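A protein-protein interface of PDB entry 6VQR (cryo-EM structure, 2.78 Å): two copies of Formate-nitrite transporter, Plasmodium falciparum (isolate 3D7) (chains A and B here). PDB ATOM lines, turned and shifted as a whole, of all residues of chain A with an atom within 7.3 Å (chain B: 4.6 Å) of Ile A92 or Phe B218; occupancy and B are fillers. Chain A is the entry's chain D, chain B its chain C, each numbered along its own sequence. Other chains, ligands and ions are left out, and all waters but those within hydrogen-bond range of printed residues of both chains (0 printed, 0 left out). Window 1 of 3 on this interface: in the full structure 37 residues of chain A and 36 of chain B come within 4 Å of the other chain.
Phe A214 touches its own counterpart, Phe B214.
4 positions are printed for both chains.
Of the 10 printed residues of chain B, 5 touch a printed residue of chain A.
Printed residues of chain B that touch a printed residue of chain A: Phe B195, Phe B214, Phe B218, Tyr B221 and Ala B222.
Hydrophobic or aromatic side chains of chain B within 4 Å of the printed part of chain A: Phe B195, Phe B214, Phe B218, Tyr B221 and Ala B222.
Of the 21 printed residues of chain A, 7 touch a printed residue of chain B.
Printed residues of chain A that touch a printed residue of chain B: Leu A56, Ala A60, Phe A88, Thr A89, Ile A92, Val A213 and Phe A214.
Hydrophobic or aromatic side chains of chain A that line the printed part of chain B: Leu A56, Ala A60, Phe A88, Ile A92, Val A213 and Phe A214.
Among the printed residues, 9 pairs touch across the chains.
Among the printed residues, merely in contact across the chains: Leu A56 with Phe B195 (3.5 Å), Ala A60 with Ala B222 (3.95 Å), Phe A88 with Tyr B221 (3.4 Å), Thr A89 with Tyr B221 (3.4 Å), Thr A89 with Ala B222 (3.7 Å), Ile A92 with Phe B195 (3.7 Å), Ile A92 with Phe B218 (3.97 Å), Val A213 with Phe B218 (3.9 Å) and Phe A214 with Phe B214 (3.3 Å).
OG of Ser A61 sits at hydrogen-bond distance from O of Thr A89 (3.5 Å).
The side-chain sulfur (SG) of Cys A96 lies within hydrogen-bond range of the backbone carbonyl oxygen (O) of Ile A92, at 3.3 Å.
Of chain B, only Phe B195 and Phe B218 come within 4 Å of Ile A92.
Phe B218 touches two residues of chain A.
Printed residues of chain A within 4 Å of Ala B222: Ala A60 and Thr A89.
Of the printed residues of chain B, Ala A60 touches Ala B222.
The nearest residue of chain B that does not touch Ile A92 is Ala B219 (4.4 Å).
The nearest printed residue of chain A that does not touch Phe B195 is Ala A60 (4.2 Å).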
ATOM      1  N   PHE A  53      13.195   7.124 -25.057  1.00  0.00           N
ATOM      2  CA  PHE A  53      12.744   5.733 -25.068  1.00  0.00           C
ATOM      3  C   PHE A  53      13.731   4.828 -24.343  1.00  0.00           C
ATOM      4  O   PHE A  53      13.335   3.952 -23.559  1.00  0.00           O
ATOM      5  CB  PHE A  53      12.545   5.254 -26.503  1.00  0.00           C
ATOM      6  CG  PHE A  53      11.358   5.846 -27.174  1.00  0.00           C
ATOM      7  CD1 PHE A  53      10.441   6.581 -26.456  1.00  0.00           C
ATOM      8  CD2 PHE A  53      11.159   5.676 -28.522  1.00  0.00           C
ATOM      9  CE1 PHE A  53       9.346   7.136 -27.071  1.00  0.00           C
ATOM     10  CE2 PHE A  53      10.067   6.227 -29.143  1.00  0.00           C
ATOM     11  CZ  PHE A  53       9.161   6.961 -28.416  1.00  0.00           C
ATOM     12  N   LEU A  56      13.336   5.254 -20.689  1.00  0.00           N
ATOM     13  CA  LEU A  56      12.143   4.599 -20.170  1.00  0.00           C
ATOM     14  C   LEU A  56      12.389   3.114 -19.956  1.00  0.00           C
ATOM     15  O   LEU A  56      12.177   2.582 -18.858  1.00  0.00           O
ATOM     16  CB  LEU A  56      10.974   4.813 -21.127  1.00  0.00           C
ATOM     17  CG  LEU A  56       9.622   4.303 -20.642  1.00  0.00           C
ATOM     18  CD1 LEU A  56       9.479   4.525 -19.159  1.00  0.00           C
ATOM     19  CD2 LEU A  56       8.505   4.989 -21.381  1.00  0.00           C
ATOM     20  N   CYS A  57      12.826   2.424 -21.008  1.00  0.00           N
ATOM     21  CA  CYS A  57      12.991   0.981 -20.888  1.00  0.00           C
ATOM     22  C   CYS A  57      14.090   0.620 -19.900  1.00  0.00           C
ATOM     23  O   CYS A  57      14.009  -0.426 -19.246  1.00  0.00           O
ATOM     24  CB  CYS A  57      13.246   0.375 -22.258  1.00  0.00           C
ATOM     25  SG  CYS A  57      12.161   1.085 -23.500  1.00  0.00           S
ATOM     26  N   ALA A  60      12.503   0.907 -16.419  1.00  0.00           N
ATOM     27  CA  ALA A  60      11.650  -0.262 -16.233  1.00  0.00           C
ATOM     28  C   ALA A  60      12.475  -1.493 -15.884  1.00  0.00           C
ATOM     29  O   ALA A  60      12.178  -2.211 -14.917  1.00  0.00           O
ATOM     30  CB  ALA A  60      10.826  -0.505 -17.495  1.00  0.00           C
ATOM     31  N   SER A  61      13.528  -1.748 -16.661  1.00  0.00           N
ATOM     32  CA  SER A  61      14.339  -2.935 -16.432  1.00  0.00           C
ATOM     33  C   SER A  61      15.066  -2.866 -15.098  1.00  0.00           C
ATOM     34  O   SER A  61      15.238  -3.888 -14.425  1.00  0.00           O
ATOM     35  CB  SER A  61      15.320  -3.106 -17.580  1.00  0.00           C
ATOM     36  OG  SER A  61      14.707  -2.736 -18.797  1.00  0.00           O
ATOM     37  N   PHE A  88      15.325  -9.612 -19.817  1.00  0.00           N
ATOM     38  CA  PHE A  88      14.016  -9.961 -20.348  1.00  0.00           C
ATOM     39  C   PHE A  88      13.143  -8.738 -20.583  1.00  0.00           C
ATOM     40  O   PHE A  88      12.417  -8.681 -21.577  1.00  0.00           O
ATOM     41  CB  PHE A  88      13.307 -10.928 -19.403  1.00  0.00           C
ATOM     42  CG  PHE A  88      11.968 -11.375 -19.894  1.00  0.00           C
ATOM     43  CD1 PHE A  88      11.866 -12.365 -20.852  1.00  0.00           C
ATOM     44  CD2 PHE A  88      10.809 -10.809 -19.397  1.00  0.00           C
ATOM     45  CE1 PHE A  88      10.633 -12.780 -21.309  1.00  0.00           C
ATOM     46  CE2 PHE A  88       9.574 -11.220 -19.850  1.00  0.00           C
ATOM     47  CZ  PHE A  88       9.486 -12.207 -20.806  1.00  0.00           C
ATOM     48  N   THR A  89      13.194  -7.754 -19.692  1.00  0.00           N
ATOM     49  CA  THR A  89      12.309  -6.603 -19.805  1.00  0.00           C
ATOM     50  C   THR A  89      12.952  -5.409 -20.491  1.00  0.00           C
ATOM     51  O   THR A  89      12.284  -4.386 -20.663  1.00  0.00           O
ATOM     52  CB  THR A  89      11.793  -6.172 -18.430  1.00  0.00           C
ATOM     53  OG1 THR A  89      11.010  -4.982 -18.570  1.00  0.00           O
ATOM     54  CG2 THR A  89      12.930  -5.880 -17.512  1.00  0.00           C
ATOM     55  N   PHE A  90      14.221  -5.493 -20.864  1.00  0.00           N
ATOM     56  CA  PHE A  90      14.819  -4.415 -21.644  1.00  0.00           C
ATOM     57  C   PHE A  90      14.506  -4.481 -23.140  1.00  0.00           C
ATOM     58  O   PHE A  90      14.213  -3.441 -23.741  1.00  0.00           O
ATOM     59  CB  PHE A  90      16.333  -4.394 -21.444  1.00  0.00           C
ATOM     60  CG  PHE A  90      17.000  -3.177 -22.010  1.00  0.00           C
ATOM     61  CD1 PHE A  90      17.012  -1.994 -21.311  1.00  0.00           C
ATOM     62  CD2 PHE A  90      17.619  -3.220 -23.240  1.00  0.00           C
ATOM     63  CE1 PHE A  90      17.620  -0.881 -21.823  1.00  0.00           C
ATOM     64  CE2 PHE A  90      18.230  -2.105 -23.756  1.00  0.00           C
ATOM     65  CZ  PHE A  90      18.229  -0.935 -23.048  1.00  0.00           C
ATOM     66  N   PRO A  91      14.558  -5.658 -23.795  1.00  0.00           N
ATOM     67  CA  PRO A  91      14.519  -5.666 -25.264  1.00  0.00           C
ATOM     68  C   PRO A  91      13.191  -5.256 -25.878  1.00  0.00           C
ATOM     69  O   PRO A  91      12.649  -5.985 -26.713  1.00  0.00           O
ATOM     70  CB  PRO A  91      14.832  -7.126 -25.607  1.00  0.00           C
ATOM     71  CG  PRO A  91      15.451  -7.683 -24.402  1.00  0.00           C
ATOM     72  CD  PRO A  91      14.775  -7.017 -23.280  1.00  0.00           C
ATOM     73  N   ILE A  92      12.659  -4.099 -25.496  1.00  0.00           N
ATOM     74  CA  ILE A  92      11.428  -3.607 -26.101  1.00  0.00           C
ATOM     75  C   ILE A  92      11.673  -2.195 -26.600  1.00  0.00           C
ATOM     76  O   ILE A  92      10.879  -1.652 -27.375  1.00  0.00           O
ATOM     77  CB  ILE A  92      10.245  -3.657 -25.117  1.00  0.00           C
ATOM     78  CG1 ILE A  92      10.119  -2.338 -24.356  1.00  0.00           C
ATOM     79  CG2 ILE A  92      10.399  -4.813 -24.143  1.00  0.00           C
ATOM     80  CD1 ILE A  92       8.834  -1.595 -24.632  1.00  0.00           C
ATOM     81  N   ALA A  93      12.780  -1.591 -26.157  1.00  0.00           N
ATOM     82  CA  ALA A  93      13.125  -0.245 -26.604  1.00  0.00           C
ATOM     83  C   ALA A  93      13.237  -0.180 -28.118  1.00  0.00           C
ATOM     84  O   ALA A  93      12.856   0.819 -28.733  1.00  0.00           O
ATOM     85  CB  ALA A  93      14.433   0.205 -25.958  1.00  0.00           C
ATOM     86  N   PHE A  94      13.764  -1.237 -28.732  1.00  0.00           N
ATOM     87  CA  PHE A  94      13.926  -1.261 -30.179  1.00  0.00           C
ATOM     88  C   PHE A  94      12.605  -1.013 -30.885  1.00  0.00           C
ATOM     89  O   PHE A  94      12.557  -0.280 -31.878  1.00  0.00           O
ATOM     90  CB  PHE A  94      14.520  -2.600 -30.601  1.00  0.00           C
ATOM     91  CG  PHE A  94      15.076  -2.614 -31.993  1.00  0.00           C
ATOM     92  CD1 PHE A  94      14.256  -2.861 -33.080  1.00  0.00           C
ATOM     93  CD2 PHE A  94      16.426  -2.420 -32.214  1.00  0.00           C
ATOM     94  CE1 PHE A  94      14.768  -2.887 -34.360  1.00  0.00           C
ATOM     95  CE2 PHE A  94      16.943  -2.448 -33.491  1.00  0.00           C
ATOM     96  CZ  PHE A  94      16.114  -2.679 -34.565  1.00  0.00           C
ATOM     97  N   MET A  95      11.521  -1.607 -30.387  1.00  0.00           N
ATOM     98  CA  MET A  95      10.229  -1.459 -31.047  1.00  0.00           C
ATOM     99  C   MET A  95       9.760  -0.012 -31.019  1.00  0.00           C
ATOM    100  O   MET A  95       9.356   0.541 -32.048  1.00  0.00           O
ATOM    101  CB  MET A  95       9.195  -2.366 -30.388  1.00  0.00           C
ATOM    102  CG  MET A  95       8.320  -3.097 -31.377  1.00  0.00           C
ATOM    103  SD  MET A  95       9.196  -4.446 -32.181  1.00  0.00           S
ATOM    104  CE  MET A  95      10.189  -5.045 -30.819  1.00  0.00           C
ATOM    105  N   CYS A  96       9.800   0.620 -29.848  1.00  0.00           N
ATOM    106  CA  CYS A  96       9.384   2.013 -29.777  1.00  0.00           C
ATOM    107  C   CYS A  96      10.306   2.922 -30.576  1.00  0.00           C
ATOM    108  O   CYS A  96       9.846   3.916 -31.144  1.00  0.00           O
ATOM    109  CB  CYS A  96       9.284   2.472 -28.323  1.00  0.00           C
ATOM    110  SG  CYS A  96      10.358   1.641 -27.161  1.00  0.00           S
ATOM    111  N   ILE A  97      11.595   2.603 -30.657  1.00  0.00           N
ATOM    112  CA  ILE A  97      12.476   3.471 -31.425  1.00  0.00           C
ATOM    113  C   ILE A  97      12.267   3.292 -32.927  1.00  0.00           C
ATOM    114  O   ILE A  97      12.433   4.248 -33.691  1.00  0.00           O
ATOM    115  CB  ILE A  97      13.940   3.242 -31.020  1.00  0.00           C
ATOM    116  CG1 ILE A  97      14.110   3.479 -29.525  1.00  0.00           C
ATOM    117  CG2 ILE A  97      14.862   4.172 -31.777  1.00  0.00           C
ATOM    118  CD1 ILE A  97      15.393   2.923 -28.971  1.00  0.00           C
ATOM    119  N   ILE A  98      11.878   2.104 -33.386  1.00  0.00           N
ATOM    120  CA  ILE A  98      11.713   1.924 -34.826  1.00  0.00           C
ATOM    121  C   ILE A  98      10.337   2.389 -35.285  1.00  0.00           C
ATOM    122  O   ILE A  98      10.224   3.208 -36.202  1.00  0.00           O
ATOM    123  CB  ILE A  98      11.990   0.467 -35.249  1.00  0.00           C
ATOM    124  CG1 ILE A  98      11.743   0.312 -36.745  1.00  0.00           C
ATOM    125  CG2 ILE A  98      11.119  -0.518 -34.512  1.00  0.00           C
ATOM    126  CD1 ILE A  98      11.846  -1.104 -37.218  1.00  0.00           C
ATOM    127  N   VAL A 213       9.501  -8.613 -33.720  1.00  0.00           N
ATOM    128  CA  VAL A 213       9.496  -8.586 -32.263  1.00  0.00           C
ATOM    129  C   VAL A 213      10.447  -9.633 -31.709  1.00  0.00           C
ATOM    130  O   VAL A 213      11.352  -9.319 -30.930  1.00  0.00           O
ATOM    131  CB  VAL A 213       8.067  -8.783 -31.727  1.00  0.00           C
ATOM    132  CG1 VAL A 213       8.101  -9.059 -30.242  1.00  0.00           C
ATOM    133  CG2 VAL A 213       7.228  -7.559 -32.017  1.00  0.00           C
ATOM    134  N   PHE A 214      10.282 -10.885 -32.131  1.00  0.00           N
ATOM    135  CA  PHE A 214      11.018 -11.970 -31.501  1.00  0.00           C
ATOM    136  C   PHE A 214      12.491 -11.950 -31.879  1.00  0.00           C
ATOM    137  O   PHE A 214      13.350 -12.224 -31.033  1.00  0.00           O
ATOM    138  CB  PHE A 214      10.373 -13.299 -31.863  1.00  0.00           C
ATOM    139  CG  PHE A 214       8.994 -13.452 -31.311  1.00  0.00           C
ATOM    140  CD1 PHE A 214       8.778 -13.412 -29.947  1.00  0.00           C
ATOM    141  CD2 PHE A 214       7.910 -13.607 -32.150  1.00  0.00           C
ATOM    142  CE1 PHE A 214       7.514 -13.541 -29.434  1.00  0.00           C
ATOM    143  CE2 PHE A 214       6.641 -13.738 -31.639  1.00  0.00           C
ATOM    144  CZ  PHE A 214       6.446 -13.707 -30.281  1.00  0.00           C
ATOM    145  N   VAL A 216      14.415  -9.283 -32.716  1.00  0.00           N
ATOM    146  CA  VAL A 216      15.150  -8.257 -31.998  1.00  0.00           C
ATOM    147  C   VAL A 216      15.124  -8.536 -30.503  1.00  0.00           C
ATOM    148  O   VAL A 216      16.063  -8.170 -29.785  1.00  0.00           O
ATOM    149  CB  VAL A 216      14.616  -6.854 -32.322  1.00  0.00           C
ATOM    150  CG1 VAL A 216      13.202  -6.686 -31.817  1.00  0.00           C
ATOM    151  CG2 VAL A 216      15.538  -5.816 -31.735  1.00  0.00           C
ATOM    152  N   PHE A 217      14.089  -9.215 -30.003  1.00  0.00           N
ATOM    153  CA  PHE A 217      14.077  -9.570 -28.591  1.00  0.00           C
ATOM    154  C   PHE A 217      15.230 -10.497 -28.261  1.00  0.00           C
ATOM    155  O   PHE A 217      15.966 -10.268 -27.301  1.00  0.00           O
ATOM    156  CB  PHE A 217      12.756 -10.232 -28.204  1.00  0.00           C
ATOM    157  CG  PHE A 217      12.837 -11.010 -26.922  1.00  0.00           C
ATOM    158  CD1 PHE A 217      12.774 -10.363 -25.705  1.00  0.00           C
ATOM    159  CD2 PHE A 217      13.003 -12.381 -26.934  1.00  0.00           C
ATOM    160  CE1 PHE A 217      12.862 -11.067 -24.530  1.00  0.00           C
ATOM    161  CE2 PHE A 217      13.092 -13.085 -25.760  1.00  0.00           C
ATOM    162  CZ  PHE A 217      13.019 -12.426 -24.555  1.00  0.00           C
ATOM    163  N   VAL A 220      18.641  -8.479 -28.432  1.00  0.00           N
ATOM    164  CA  VAL A 220      18.909  -7.535 -27.354  1.00  0.00           C
ATOM    165  C   VAL A 220      18.977  -8.243 -26.012  1.00  0.00           C
ATOM    166  O   VAL A 220      19.713  -7.815 -25.117  1.00  0.00           O
ATOM    167  CB  VAL A 220      17.864  -6.409 -27.346  1.00  0.00           C
ATOM    168  CG1 VAL A 220      18.255  -5.340 -26.351  1.00  0.00           C
ATOM    169  CG2 VAL A 220      17.753  -5.797 -28.722  1.00  0.00           C
ATOM    170  N   PHE B 195       4.236   4.638 -21.955  1.00  0.00           N
ATOM    171  CA  PHE B 195       4.211   3.226 -22.341  1.00  0.00           C
ATOM    172  C   PHE B 195       2.935   2.855 -23.087  1.00  0.00           C
ATOM    173  O   PHE B 195       2.988   2.196 -24.134  1.00  0.00           O
ATOM    174  CB  PHE B 195       4.364   2.326 -21.119  1.00  0.00           C
ATOM    175  CG  PHE B 195       5.734   1.752 -20.954  1.00  0.00           C
ATOM    176  CD1 PHE B 195       6.205   0.813 -21.850  1.00  0.00           C
ATOM    177  CD2 PHE B 195       6.521   2.091 -19.880  1.00  0.00           C
ATOM    178  CE1 PHE B 195       7.449   0.260 -21.704  1.00  0.00           C
ATOM    179  CE2 PHE B 195       7.764   1.529 -19.727  1.00  0.00           C
ATOM    180  CZ  PHE B 195       8.228   0.618 -20.643  1.00  0.00           C
ATOM    181  N   PHE B 214       2.006  -9.616 -29.240  1.00  0.00           N
ATOM    182  CA  PHE B 214       3.246  -9.667 -28.472  1.00  0.00           C
ATOM    183  C   PHE B 214       3.839  -8.289 -28.207  1.00  0.00           C
ATOM    184  O   PHE B 214       4.410  -8.059 -27.134  1.00  0.00           O
ATOM    185  CB  PHE B 214       4.248 -10.569 -29.176  1.00  0.00           C
ATOM    186  CG  PHE B 214       4.022 -12.016 -28.897  1.00  0.00           C
ATOM    187  CD1 PHE B 214       4.556 -12.605 -27.768  1.00  0.00           C
ATOM    188  CD2 PHE B 214       3.238 -12.780 -29.738  1.00  0.00           C
ATOM    189  CE1 PHE B 214       4.336 -13.936 -27.502  1.00  0.00           C
ATOM    190  CE2 PHE B 214       3.013 -14.107 -29.476  1.00  0.00           C
ATOM    191  CZ  PHE B 214       3.564 -14.688 -28.357  1.00  0.00           C
ATOM    192  N   SER B 215       3.732  -7.363 -29.157  1.00  0.00           N
ATOM    193  CA  SER B 215       4.192  -6.005 -28.903  1.00  0.00           C
ATOM    194  C   SER B 215       3.469  -5.410 -27.705  1.00  0.00           C
ATOM    195  O   SER B 215       4.098  -4.865 -26.790  1.00  0.00           O
ATOM    196  CB  SER B 215       3.981  -5.143 -30.146  1.00  0.00           C
ATOM    197  OG  SER B 215       2.733  -4.479 -30.092  1.00  0.00           O
ATOM    198  N   VAL B 216       2.141  -5.522 -27.687  1.00  0.00           N
ATOM    199  CA  VAL B 216       1.380  -4.973 -26.573  1.00  0.00           C
ATOM    200  C   VAL B 216       1.632  -5.774 -25.306  1.00  0.00           C
ATOM    201  O   VAL B 216       1.620  -5.214 -24.201  1.00  0.00           O
ATOM    202  CB  VAL B 216      -0.114  -4.900 -26.935  1.00  0.00           C
ATOM    203  CG1 VAL B 216      -0.279  -4.315 -28.330  1.00  0.00           C
ATOM    204  CG2 VAL B 216      -0.767  -6.262 -26.849  1.00  0.00           C
ATOM    205  N   PHE B 217       1.920  -7.072 -25.435  1.00  0.00           N
ATOM    206  CA  PHE B 217       2.295  -7.866 -24.271  1.00  0.00           C
ATOM    207  C   PHE B 217       3.526  -7.283 -23.597  1.00  0.00           C
ATOM    208  O   PHE B 217       3.507  -6.964 -22.405  1.00  0.00           O
ATOM    209  CB  PHE B 217       2.548  -9.316 -24.685  1.00  0.00           C
ATOM    210  CG  PHE B 217       3.110 -10.161 -23.585  1.00  0.00           C
ATOM    211  CD1 PHE B 217       2.290 -10.658 -22.591  1.00  0.00           C
ATOM    212  CD2 PHE B 217       4.458 -10.448 -23.535  1.00  0.00           C
ATOM    213  CE1 PHE B 217       2.799 -11.426 -21.570  1.00  0.00           C
ATOM    214  CE2 PHE B 217       4.977 -11.216 -22.516  1.00  0.00           C
ATOM    215  CZ  PHE B 217       4.144 -11.707 -21.532  1.00  0.00           C
ATOM    216  N   PHE B 218       4.613  -7.148 -24.353  1.00  0.00           N
ATOM    217  CA  PHE B 218       5.853  -6.643 -23.775  1.00  0.00           C
ATOM    218  C   PHE B 218       5.685  -5.222 -23.256  1.00  0.00           C
ATOM    219  O   PHE B 218       6.156  -4.898 -22.159  1.00  0.00           O
ATOM    220  CB  PHE B 218       6.977  -6.716 -24.803  1.00  0.00           C
ATOM    221  CG  PHE B 218       7.486  -8.102 -25.037  1.00  0.00           C
ATOM    222  CD1 PHE B 218       8.053  -8.823 -24.007  1.00  0.00           C
ATOM    223  CD2 PHE B 218       7.390  -8.687 -26.282  1.00  0.00           C
ATOM    224  CE1 PHE B 218       8.520 -10.101 -24.215  1.00  0.00           C
ATOM    225  CE2 PHE B 218       7.854  -9.965 -26.497  1.00  0.00           C
ATOM    226  CZ  PHE B 218       8.419 -10.673 -25.461  1.00  0.00           C
ATOM    227  N   ALA B 219       4.996  -4.367 -24.015  1.00  0.00           N
ATOM    228  CA  ALA B 219       4.801  -2.988 -23.578  1.00  0.00           C
ATOM    229  C   ALA B 219       4.078  -2.924 -22.237  1.00  0.00           C
ATOM    230  O   ALA B 219       4.556  -2.285 -21.289  1.00  0.00           O
ATOM    231  CB  ALA B 219       4.036  -2.209 -24.647  1.00  0.00           C
ATOM    232  N   VAL B 220       2.931  -3.602 -22.122  1.00  0.00           N
ATOM    233  CA  VAL B 220       2.133  -3.470 -20.907  1.00  0.00           C
ATOM    234  C   VAL B 220       2.766  -4.219 -19.747  1.00  0.00           C
ATOM    235  O   VAL B 220       2.666  -3.781 -18.596  1.00  0.00           O
ATOM    236  CB  VAL B 220       0.692  -3.936 -21.162  1.00  0.00           C
ATOM    237  CG1 VAL B 220      -0.120  -3.873 -19.881  1.00  0.00           C
ATOM    238  CG2 VAL B 220       0.058  -3.074 -22.237  1.00  0.00           C
ATOM    239  N   TYR B 221       3.441  -5.339 -20.009  1.00  0.00           N
ATOM    240  CA  TYR B 221       4.152  -6.022 -18.936  1.00  0.00           C
ATOM    241  C   TYR B 221       5.237  -5.127 -18.359  1.00  0.00           C
ATOM    242  O   TYR B 221       5.353  -4.980 -17.136  1.00  0.00           O
ATOM    243  CB  TYR B 221       4.752  -7.332 -19.443  1.00  0.00           C
ATOM    244  CG  TYR B 221       6.082  -7.662 -18.812  1.00  0.00           C
ATOM    245  CD1 TYR B 221       6.167  -8.049 -17.485  1.00  0.00           C
ATOM    246  CD2 TYR B 221       7.255  -7.574 -19.542  1.00  0.00           C
ATOM    247  CE1 TYR B 221       7.377  -8.336 -16.906  1.00  0.00           C
ATOM    248  CE2 TYR B 221       8.471  -7.865 -18.971  1.00  0.00           C
ATOM    249  CZ  TYR B 221       8.527  -8.245 -17.653  1.00  0.00           C
ATOM    250  OH  TYR B 221       9.741  -8.537 -17.078  1.00  0.00           O
ATOM    251  N   ALA B 222       6.057  -4.533 -19.227  1.00  0.00           N
ATOM    252  CA  ALA B 222       7.116  -3.661 -18.743  1.00  0.00           C
ATOM    253  C   ALA B 222       6.546  -2.451 -18.029  1.00  0.00           C
ATOM    254  O   ALA B 222       7.164  -1.937 -17.093  1.00  0.00           O
ATOM    255  CB  ALA B 222       8.010  -3.229 -19.902  1.00  0.00           C
